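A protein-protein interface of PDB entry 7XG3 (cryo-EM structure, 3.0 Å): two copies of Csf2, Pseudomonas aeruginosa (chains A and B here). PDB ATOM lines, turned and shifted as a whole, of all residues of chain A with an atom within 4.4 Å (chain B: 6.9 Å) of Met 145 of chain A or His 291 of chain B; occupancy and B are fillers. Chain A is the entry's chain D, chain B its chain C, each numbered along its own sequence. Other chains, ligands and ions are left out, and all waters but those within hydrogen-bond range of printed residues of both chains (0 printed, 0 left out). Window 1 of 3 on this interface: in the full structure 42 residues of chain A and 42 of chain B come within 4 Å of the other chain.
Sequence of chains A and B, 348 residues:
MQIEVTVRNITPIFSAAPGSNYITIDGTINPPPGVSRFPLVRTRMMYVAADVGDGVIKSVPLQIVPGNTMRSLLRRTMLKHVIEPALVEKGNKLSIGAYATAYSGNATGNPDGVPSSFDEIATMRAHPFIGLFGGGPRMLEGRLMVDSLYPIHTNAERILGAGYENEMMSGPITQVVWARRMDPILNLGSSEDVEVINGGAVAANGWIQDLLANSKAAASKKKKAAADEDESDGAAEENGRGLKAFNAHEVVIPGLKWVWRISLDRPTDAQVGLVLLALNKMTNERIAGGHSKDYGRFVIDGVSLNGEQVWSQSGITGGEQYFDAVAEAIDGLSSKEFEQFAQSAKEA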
ATOM      1  N   GLY A 142     -27.591   5.199   9.672  1.00  0.00           N
ATOM      2  CA  GLY A 142     -26.392   4.605   9.117  1.00  0.00           C
ATOM      3  C   GLY A 142     -25.884   3.471   9.995  1.00  0.00           C
ATOM      4  O   GLY A 142     -25.837   3.577  11.219  1.00  0.00           O
ATOM      5  N   ARG A 143     -25.511   2.367   9.345  1.00  0.00           N
ATOM      6  CA  ARG A 143     -24.927   1.240  10.063  1.00  0.00           C
ATOM      7  C   ARG A 143     -23.550   1.577  10.615  1.00  0.00           C
ATOM      8  O   ARG A 143     -23.170   1.063  11.672  1.00  0.00           O
ATOM      9  CB  ARG A 143     -24.845   0.020   9.140  1.00  0.00           C
ATOM     10  CG  ARG A 143     -24.426  -1.270   9.811  1.00  0.00           C
ATOM     11  CD  ARG A 143     -25.026  -2.481   9.125  1.00  0.00           C
ATOM     12  NE  ARG A 143     -26.470  -2.387   8.950  1.00  0.00           N
ATOM     13  CZ  ARG A 143     -27.254  -3.424   8.689  1.00  0.00           C
ATOM     14  NH1 ARG A 143     -26.767  -4.648   8.583  1.00  0.00           N
ATOM     15  NH2 ARG A 143     -28.559  -3.229   8.532  1.00  0.00           N
ATOM     16  N   LEU A 144     -22.811   2.452   9.944  1.00  0.00           N
ATOM     17  CA  LEU A 144     -21.466   2.817  10.358  1.00  0.00           C
ATOM     18  C   LEU A 144     -21.532   3.756  11.552  1.00  0.00           C
ATOM     19  O   LEU A 144     -22.239   4.767  11.518  1.00  0.00           O
ATOM     20  CB  LEU A 144     -20.697   3.487   9.219  1.00  0.00           C
ATOM     21  CG  LEU A 144     -19.189   3.248   9.158  1.00  0.00           C
ATOM     22  CD1 LEU A 144     -18.872   1.826   9.502  1.00  0.00           C
ATOM     23  CD2 LEU A 144     -18.644   3.572   7.796  1.00  0.00           C
ATOM     24  N   MET A 145     -20.814   3.403  12.608  1.00  0.00           N
ATOM     25  CA  MET A 145     -20.509   4.291  13.714  1.00  0.00           C
ATOM     26  C   MET A 145     -19.035   4.642  13.599  1.00  0.00           C
ATOM     27  O   MET A 145     -18.190   3.745  13.596  1.00  0.00           O
ATOM     28  CB  MET A 145     -20.774   3.599  15.050  1.00  0.00           C
ATOM     29  CG  MET A 145     -22.170   3.721  15.607  1.00  0.00           C
ATOM     30  SD  MET A 145     -22.660   2.230  16.479  1.00  0.00           S
ATOM     31  CE  MET A 145     -22.594   1.057  15.135  1.00  0.00           C
ATOM     32  N   VAL A 146     -18.712   5.924  13.490  1.00  0.00           N
ATOM     33  CA  VAL A 146     -17.318   6.324  13.349  1.00  0.00           C
ATOM     34  C   VAL A 146     -16.967   7.249  14.501  1.00  0.00           C
ATOM     35  O   VAL A 146     -17.520   8.350  14.614  1.00  0.00           O
ATOM     36  CB  VAL A 146     -17.033   6.990  11.995  1.00  0.00           C
ATOM     37  CG1 VAL A 146     -15.681   7.682  12.024  1.00  0.00           C
ATOM     38  CG2 VAL A 146     -17.066   5.952  10.887  1.00  0.00           C
ATOM     39  N   ASP A 147     -16.050   6.804  15.346  1.00  0.00           N
ATOM     40  CA  ASP A 147     -15.642   7.537  16.530  1.00  0.00           C
ATOM     41  C   ASP A 147     -14.534   8.508  16.130  1.00  0.00           C
ATOM     42  O   ASP A 147     -13.871   8.324  15.107  1.00  0.00           O
ATOM     43  CB  ASP A 147     -15.194   6.532  17.605  1.00  0.00           C
ATOM     44  CG  ASP A 147     -14.550   7.177  18.818  1.00  0.00           C
ATOM     45  OD1 ASP A 147     -14.960   8.297  19.185  1.00  0.00           O
ATOM     46  OD2 ASP A 147     -13.642   6.556  19.407  1.00  0.00           O
ATOM     47  N   ARG A 261     -11.951   3.997  16.095  1.00  0.00           N
ATOM     48  CA  ARG A 261     -12.913   2.928  16.308  1.00  0.00           C
ATOM     49  C   ARG A 261     -14.082   3.086  15.347  1.00  0.00           C
ATOM     50  O   ARG A 261     -14.760   4.117  15.339  1.00  0.00           O
ATOM     51  CB  ARG A 261     -13.350   2.912  17.767  1.00  0.00           C
ATOM     52  CG  ARG A 261     -12.270   2.299  18.643  1.00  0.00           C
ATOM     53  CD  ARG A 261     -12.551   2.469  20.106  1.00  0.00           C
ATOM     54  NE  ARG A 261     -12.876   3.856  20.397  1.00  0.00           N
ATOM     55  CZ  ARG A 261     -12.607   4.456  21.546  1.00  0.00           C
ATOM     56  NH1 ARG A 261     -11.997   3.817  22.531  1.00  0.00           N
ATOM     57  NH2 ARG A 261     -12.955   5.729  21.707  1.00  0.00           N
ATOM     58  N   ILE A 262     -14.301   2.052  14.548  1.00  0.00           N
ATOM     59  CA  ILE A 262     -15.257   2.030  13.454  1.00  0.00           C
ATOM     60  C   ILE A 262     -16.213   0.878  13.745  1.00  0.00           C
ATOM     61  O   ILE A 262     -15.955  -0.271  13.374  1.00  0.00           O
ATOM     62  CB  ILE A 262     -14.555   1.858  12.101  1.00  0.00           C
ATOM     63  CG1 ILE A 262     -13.477   2.925  11.909  1.00  0.00           C
ATOM     64  CG2 ILE A 262     -15.530   1.939  10.970  1.00  0.00           C
ATOM     65  CD1 ILE A 262     -12.522   2.621  10.791  1.00  0.00           C
ATOM     66  N   SER A 263     -17.315   1.177  14.418  1.00  0.00           N
ATOM     67  CA  SER A 263     -18.276   0.165  14.821  1.00  0.00           C
ATOM     68  C   SER A 263     -19.321  -0.056  13.734  1.00  0.00           C
ATOM     69  O   SER A 263     -19.585   0.821  12.907  1.00  0.00           O
ATOM     70  CB  SER A 263     -18.964   0.566  16.125  1.00  0.00           C
ATOM     71  OG  SER A 263     -18.037   1.129  17.037  1.00  0.00           O
ATOM     72  N   LEU A 264     -19.912  -1.246  13.742  1.00  0.00           N
ATOM     73  CA  LEU A 264     -20.968  -1.612  12.802  1.00  0.00           C
ATOM     74  C   LEU A 264     -21.972  -2.483  13.543  1.00  0.00           C
ATOM     75  O   LEU A 264     -21.649  -3.616  13.915  1.00  0.00           O
ATOM     76  CB  LEU A 264     -20.405  -2.358  11.594  1.00  0.00           C
ATOM     77  CG  LEU A 264     -19.556  -1.625  10.559  1.00  0.00           C
ATOM     78  CD1 LEU A 264     -18.074  -1.755  10.865  1.00  0.00           C
ATOM     79  CD2 LEU A 264     -19.860  -2.114   9.155  1.00  0.00           C
ATOM     80  N   ASP A 265     -23.184  -1.973  13.750  1.00  0.00           N
ATOM     81  CA  ASP A 265     -24.195  -2.722  14.488  1.00  0.00           C
ATOM     82  C   ASP A 265     -24.945  -3.628  13.518  1.00  0.00           C
ATOM     83  O   ASP A 265     -25.589  -3.147  12.578  1.00  0.00           O
ATOM     84  CB  ASP A 265     -25.142  -1.783  15.236  1.00  0.00           C
ATOM     85  CG  ASP A 265     -25.657  -0.649  14.372  1.00  0.00           C
ATOM     86  OD1 ASP A 265     -25.048  -0.378  13.319  1.00  0.00           O
ATOM     87  OD2 ASP A 265     -26.680  -0.038  14.743  1.00  0.00           O
ATOM     88  N   ASN B 284     -22.479  -3.381  23.494  1.00  0.00           N
ATOM     89  CA  ASN B 284     -22.648  -3.095  22.076  1.00  0.00           C
ATOM     90  C   ASN B 284     -23.682  -2.012  21.810  1.00  0.00           C
ATOM     91  O   ASN B 284     -23.850  -1.613  20.654  1.00  0.00           O
ATOM     92  CB  ASN B 284     -23.032  -4.375  21.338  1.00  0.00           C
ATOM     93  CG  ASN B 284     -21.974  -5.447  21.456  1.00  0.00           C
ATOM     94  OD1 ASN B 284     -20.822  -5.161  21.779  1.00  0.00           O
ATOM     95  ND2 ASN B 284     -22.357  -6.691  21.200  1.00  0.00           N
ATOM     96  N   GLU B 285     -24.372  -1.530  22.837  1.00  0.00           N
ATOM     97  CA  GLU B 285     -25.404  -0.525  22.659  1.00  0.00           C
ATOM     98  C   GLU B 285     -24.807   0.878  22.744  1.00  0.00           C
ATOM     99  O   GLU B 285     -23.661   1.075  23.157  1.00  0.00           O
ATOM    100  CB  GLU B 285     -26.506  -0.719  23.694  1.00  0.00           C
ATOM    101  CG  GLU B 285     -27.265  -2.022  23.543  1.00  0.00           C
ATOM    102  CD  GLU B 285     -27.517  -2.386  22.095  1.00  0.00           C
ATOM    103  OE1 GLU B 285     -28.319  -1.686  21.443  1.00  0.00           O
ATOM    104  OE2 GLU B 285     -26.921  -3.372  21.610  1.00  0.00           O
ATOM    105  N   ARG B 286     -25.601   1.868  22.343  1.00  0.00           N
ATOM    106  CA  ARG B 286     -25.187   3.265  22.334  1.00  0.00           C
ATOM    107  C   ARG B 286     -26.244   4.098  23.035  1.00  0.00           C
ATOM    108  O   ARG B 286     -27.410   3.703  23.096  1.00  0.00           O
ATOM    109  CB  ARG B 286     -24.981   3.789  20.908  1.00  0.00           C
ATOM    110  CG  ARG B 286     -23.999   2.989  20.082  1.00  0.00           C
ATOM    111  CD  ARG B 286     -22.576   3.367  20.427  1.00  0.00           C
ATOM    112  NE  ARG B 286     -21.613   2.511  19.748  1.00  0.00           N
ATOM    113  CZ  ARG B 286     -21.223   1.327  20.197  1.00  0.00           C
ATOM    114  NH1 ARG B 286     -21.692   0.830  21.328  1.00  0.00           N
ATOM    115  NH2 ARG B 286     -20.343   0.624  19.491  1.00  0.00           N
ATOM    116  N   ALA B 288     -27.133   8.016  22.766  1.00  0.00           N
ATOM    117  CA  ALA B 288     -26.810   9.295  22.139  1.00  0.00           C
ATOM    118  C   ALA B 288     -27.895   9.715  21.159  1.00  0.00           C
ATOM    119  O   ALA B 288     -28.811   8.956  20.835  1.00  0.00           O
ATOM    120  CB  ALA B 288     -25.488   9.260  21.378  1.00  0.00           C
ATOM    121  N   GLY B 289     -27.765  10.960  20.698  1.00  0.00           N
ATOM    122  CA  GLY B 289     -28.340  11.430  19.455  1.00  0.00           C
ATOM    123  C   GLY B 289     -27.228  11.662  18.452  1.00  0.00           C
ATOM    124  O   GLY B 289     -27.260  12.607  17.658  1.00  0.00           O
ATOM    125  N   GLY B 290     -26.211  10.809  18.525  1.00  0.00           N
ATOM    126  CA  GLY B 290     -25.015  10.898  17.714  1.00  0.00           C
ATOM    127  C   GLY B 290     -24.605   9.574  17.106  1.00  0.00           C
ATOM    128  O   GLY B 290     -23.417   9.237  17.129  1.00  0.00           O
ATOM    129  N   HIS B 291     -25.577   8.798  16.613  1.00  0.00           N
ATOM    130  CA  HIS B 291     -25.309   7.433  16.160  1.00  0.00           C
ATOM    131  C   HIS B 291     -24.377   7.404  14.951  1.00  0.00           C
ATOM    132  O   HIS B 291     -23.607   6.455  14.777  1.00  0.00           O
ATOM    133  CB  HIS B 291     -26.622   6.716  15.842  1.00  0.00           C
ATOM    134  CG  HIS B 291     -26.435   5.384  15.186  1.00  0.00           C
ATOM    135  ND1 HIS B 291     -26.016   4.267  15.874  1.00  0.00           N
ATOM    136  CD2 HIS B 291     -26.584   4.998  13.897  1.00  0.00           C
ATOM    137  CE1 HIS B 291     -25.926   3.247  15.040  1.00  0.00           C
ATOM    138  NE2 HIS B 291     -26.265   3.664  13.834  1.00  0.00           N
ATOM    139  N   SER B 292     -24.426   8.436  14.106  1.00  0.00           N
ATOM    140  CA  SER B 292     -23.473   8.523  13.002  1.00  0.00           C
ATOM    141  C   SER B 292     -22.056   8.723  13.513  1.00  0.00           C
ATOM    142  O   SER B 292     -21.099   8.170  12.960  1.00  0.00           O
ATOM    143  CB  SER B 292     -23.843   9.668  12.068  1.00  0.00           C
ATOM    144  OG  SER B 292     -24.022  10.870  12.793  1.00  0.00           O
ATOM    145  N   LYS B 293     -21.907   9.498  14.580  1.00  0.00           N
ATOM    146  CA  LYS B 293     -20.594   9.862  15.077  1.00  0.00           C
ATOM    147  C   LYS B 293     -20.086   8.930  16.170  1.00  0.00           C
ATOM    148  O   LYS B 293     -19.134   9.309  16.862  1.00  0.00           O
ATOM    149  CB  LYS B 293     -20.640  11.299  15.585  1.00  0.00           C
ATOM    150  CG  LYS B 293     -20.809  12.344  14.505  1.00  0.00           C
ATOM    151  CD  LYS B 293     -21.277  13.658  15.098  1.00  0.00           C
ATOM    152  CE  LYS B 293     -22.787  13.697  15.236  1.00  0.00           C
ATOM    153  NZ  LYS B 293     -23.461  13.737  13.911  1.00  0.00           N
ATOM    154  N   ASP B 294     -20.698   7.750  16.342  1.00  0.00           N
ATOM    155  CA  ASP B 294     -20.380   6.747  17.367  1.00  0.00           C
ATOM    156  C   ASP B 294     -20.495   7.290  18.788  1.00  0.00           C
ATOM    157  O   ASP B 294     -19.903   6.730  19.709  1.00  0.00           O
ATOM    158  CB  ASP B 294     -18.988   6.126  17.153  1.00  0.00           C
ATOM    159  CG  ASP B 294     -18.872   4.705  17.698  1.00  0.00           C
ATOM    160  OD1 ASP B 294     -19.855   4.202  18.279  1.00  0.00           O
ATOM    161  OD2 ASP B 294     -17.797   4.087  17.538  1.00  0.00           O
ATOM    162  N   TYR B 295     -21.252   8.364  18.989  1.00  0.00           N
ATOM    163  CA  TYR B 295     -21.452   8.933  20.313  1.00  0.00           C
ATOM    164  C   TYR B 295     -22.236   7.969  21.192  1.00  0.00           C
ATOM    165  O   TYR B 295     -23.044   7.171  20.710  1.00  0.00           O
ATOM    166  CB  TYR B 295     -22.182  10.276  20.211  1.00  0.00           C
ATOM    167  CG  TYR B 295     -21.362  11.479  19.774  1.00  0.00           C
ATOM    168  CD1 TYR B 295     -20.152  11.341  19.110  1.00  0.00           C
ATOM    169  CD2 TYR B 295     -21.855  12.764  19.960  1.00  0.00           C
ATOM    170  CE1 TYR B 295     -19.425  12.445  18.705  1.00  0.00           C
ATOM    171  CE2 TYR B 295     -21.145  13.867  19.541  1.00  0.00           C
ATOM    172  CZ  TYR B 295     -19.931  13.704  18.917  1.00  0.00           C
ATOM    173  OH  TYR B 295     -19.222  14.808  18.507  1.00  0.00           O
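No position is printed for both chains.
Hydrophobic or aromatic side chains of chain A that line the printed part of chain B: Met 145. Of the 11 printed residues of chain B, 5 touch a printed residue of chain A. Among the printed residues, 16 pairs touch across the chains. Among the printed residues, no Asp or Glu carboxylate lies within 4 Å of a Lys or Arg side-chain nitrogen of the other chain.
The guanidinium group (NH1) of Arg 286 of chain B is in hydrogen-bond range of the backbone carbonyl oxygen (O) of Asn 284 of chain B (3.3 Å). NE of Arg 286 of chain B lies within salt-bridge range of OD1 of Asp 294 of chain B (2.8 Å). The side-chain amino group (NZ) of Lys 293 of chain B sits at hydrogen-bond distance from the side-chain hydroxyl (OG) of Ser 292 of chain B, at 3.1 Å. The backbone carbonyl oxygen (O) of Met 145 of chain A is in hydrogen-bond range of the backbone NH (N) of Ser 263 of chain A, 2.8 Å away. The side-chain carboxylate of Asp 147 of chain A is in salt-bridge range of the guanidinium group of Arg 261 of chain A (2.5 Å).
Of the printed residues of chain B, Met 145 of chain A touches Arg 286 (3.4 Å), His 291 (3.2 Å), Ser 292 (3.995 Å) and Asp 294 (3.4 Å). Printed residues of chain B within 4 Å of Asp 147 of chain A: Lys 293 and Asp 294. Of the printed residues of chain B, Arg 261 of chain A touches Asp 294 (3.7 Å). Printed residues of chain B within 4 Å of Asp 265 of chain A: His 291.
The guanidinium group of Arg 286 of chain B sits at hydrogen-bond distance from the side-chain sulfur of Met 145 of chain A. The side-chain hydroxyl (OG) of Ser 263 of chain A is in hydrogen-bond range of the guanidinium group (NH2) of Arg 286 of chain B. A ring nitrogen (NE2) of His 291 of chain B lies within hydrogen-bond range of the backbone carbonyl oxygen of Gly 142 of chain A, 2.7 Å away. The backbone carbonyl oxygen (O) of Ser 292 of chain B lies within hydrogen-bond range of the backbone NH (N) of Val 146 of chain A. OG of Ser 263 of chain A sits at hydrogen-bond distance from OD2 of Asp 294 of chain B, at 3.0 Å. The backbone carbonyl oxygen of Lys 293 of chain B lies close to the backbone carbonyl oxygen of Val 146 of chain A, at 2.9 Å.
O of His 291 of chain B touches O of Leu 144 of chain A, 3.9 Å away. Leu 144 of chain A touches Ser 292 of chain B. CG of Met 145 of chain A touches O of His 291 of chain B (3.2 Å). Ser 292 of chain B touches Met 145 of chain A. Asp 294 of chain B touches Met 145 of chain A. Val 146 of chain A touches Asp 294 of chain B (C to CB, 3.5 Å). Lys 293 of chain B touches Asp 147 of chain A. Asp 294 of chain B touches Asp 147 of chain A. Arg 261 of chain A touches Asp 294 of chain B (O to OD2, 3.7 Å). OD2 of Asp 265 of chain A touches CE1 of His 291 of chain B, at 3.4 Å.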
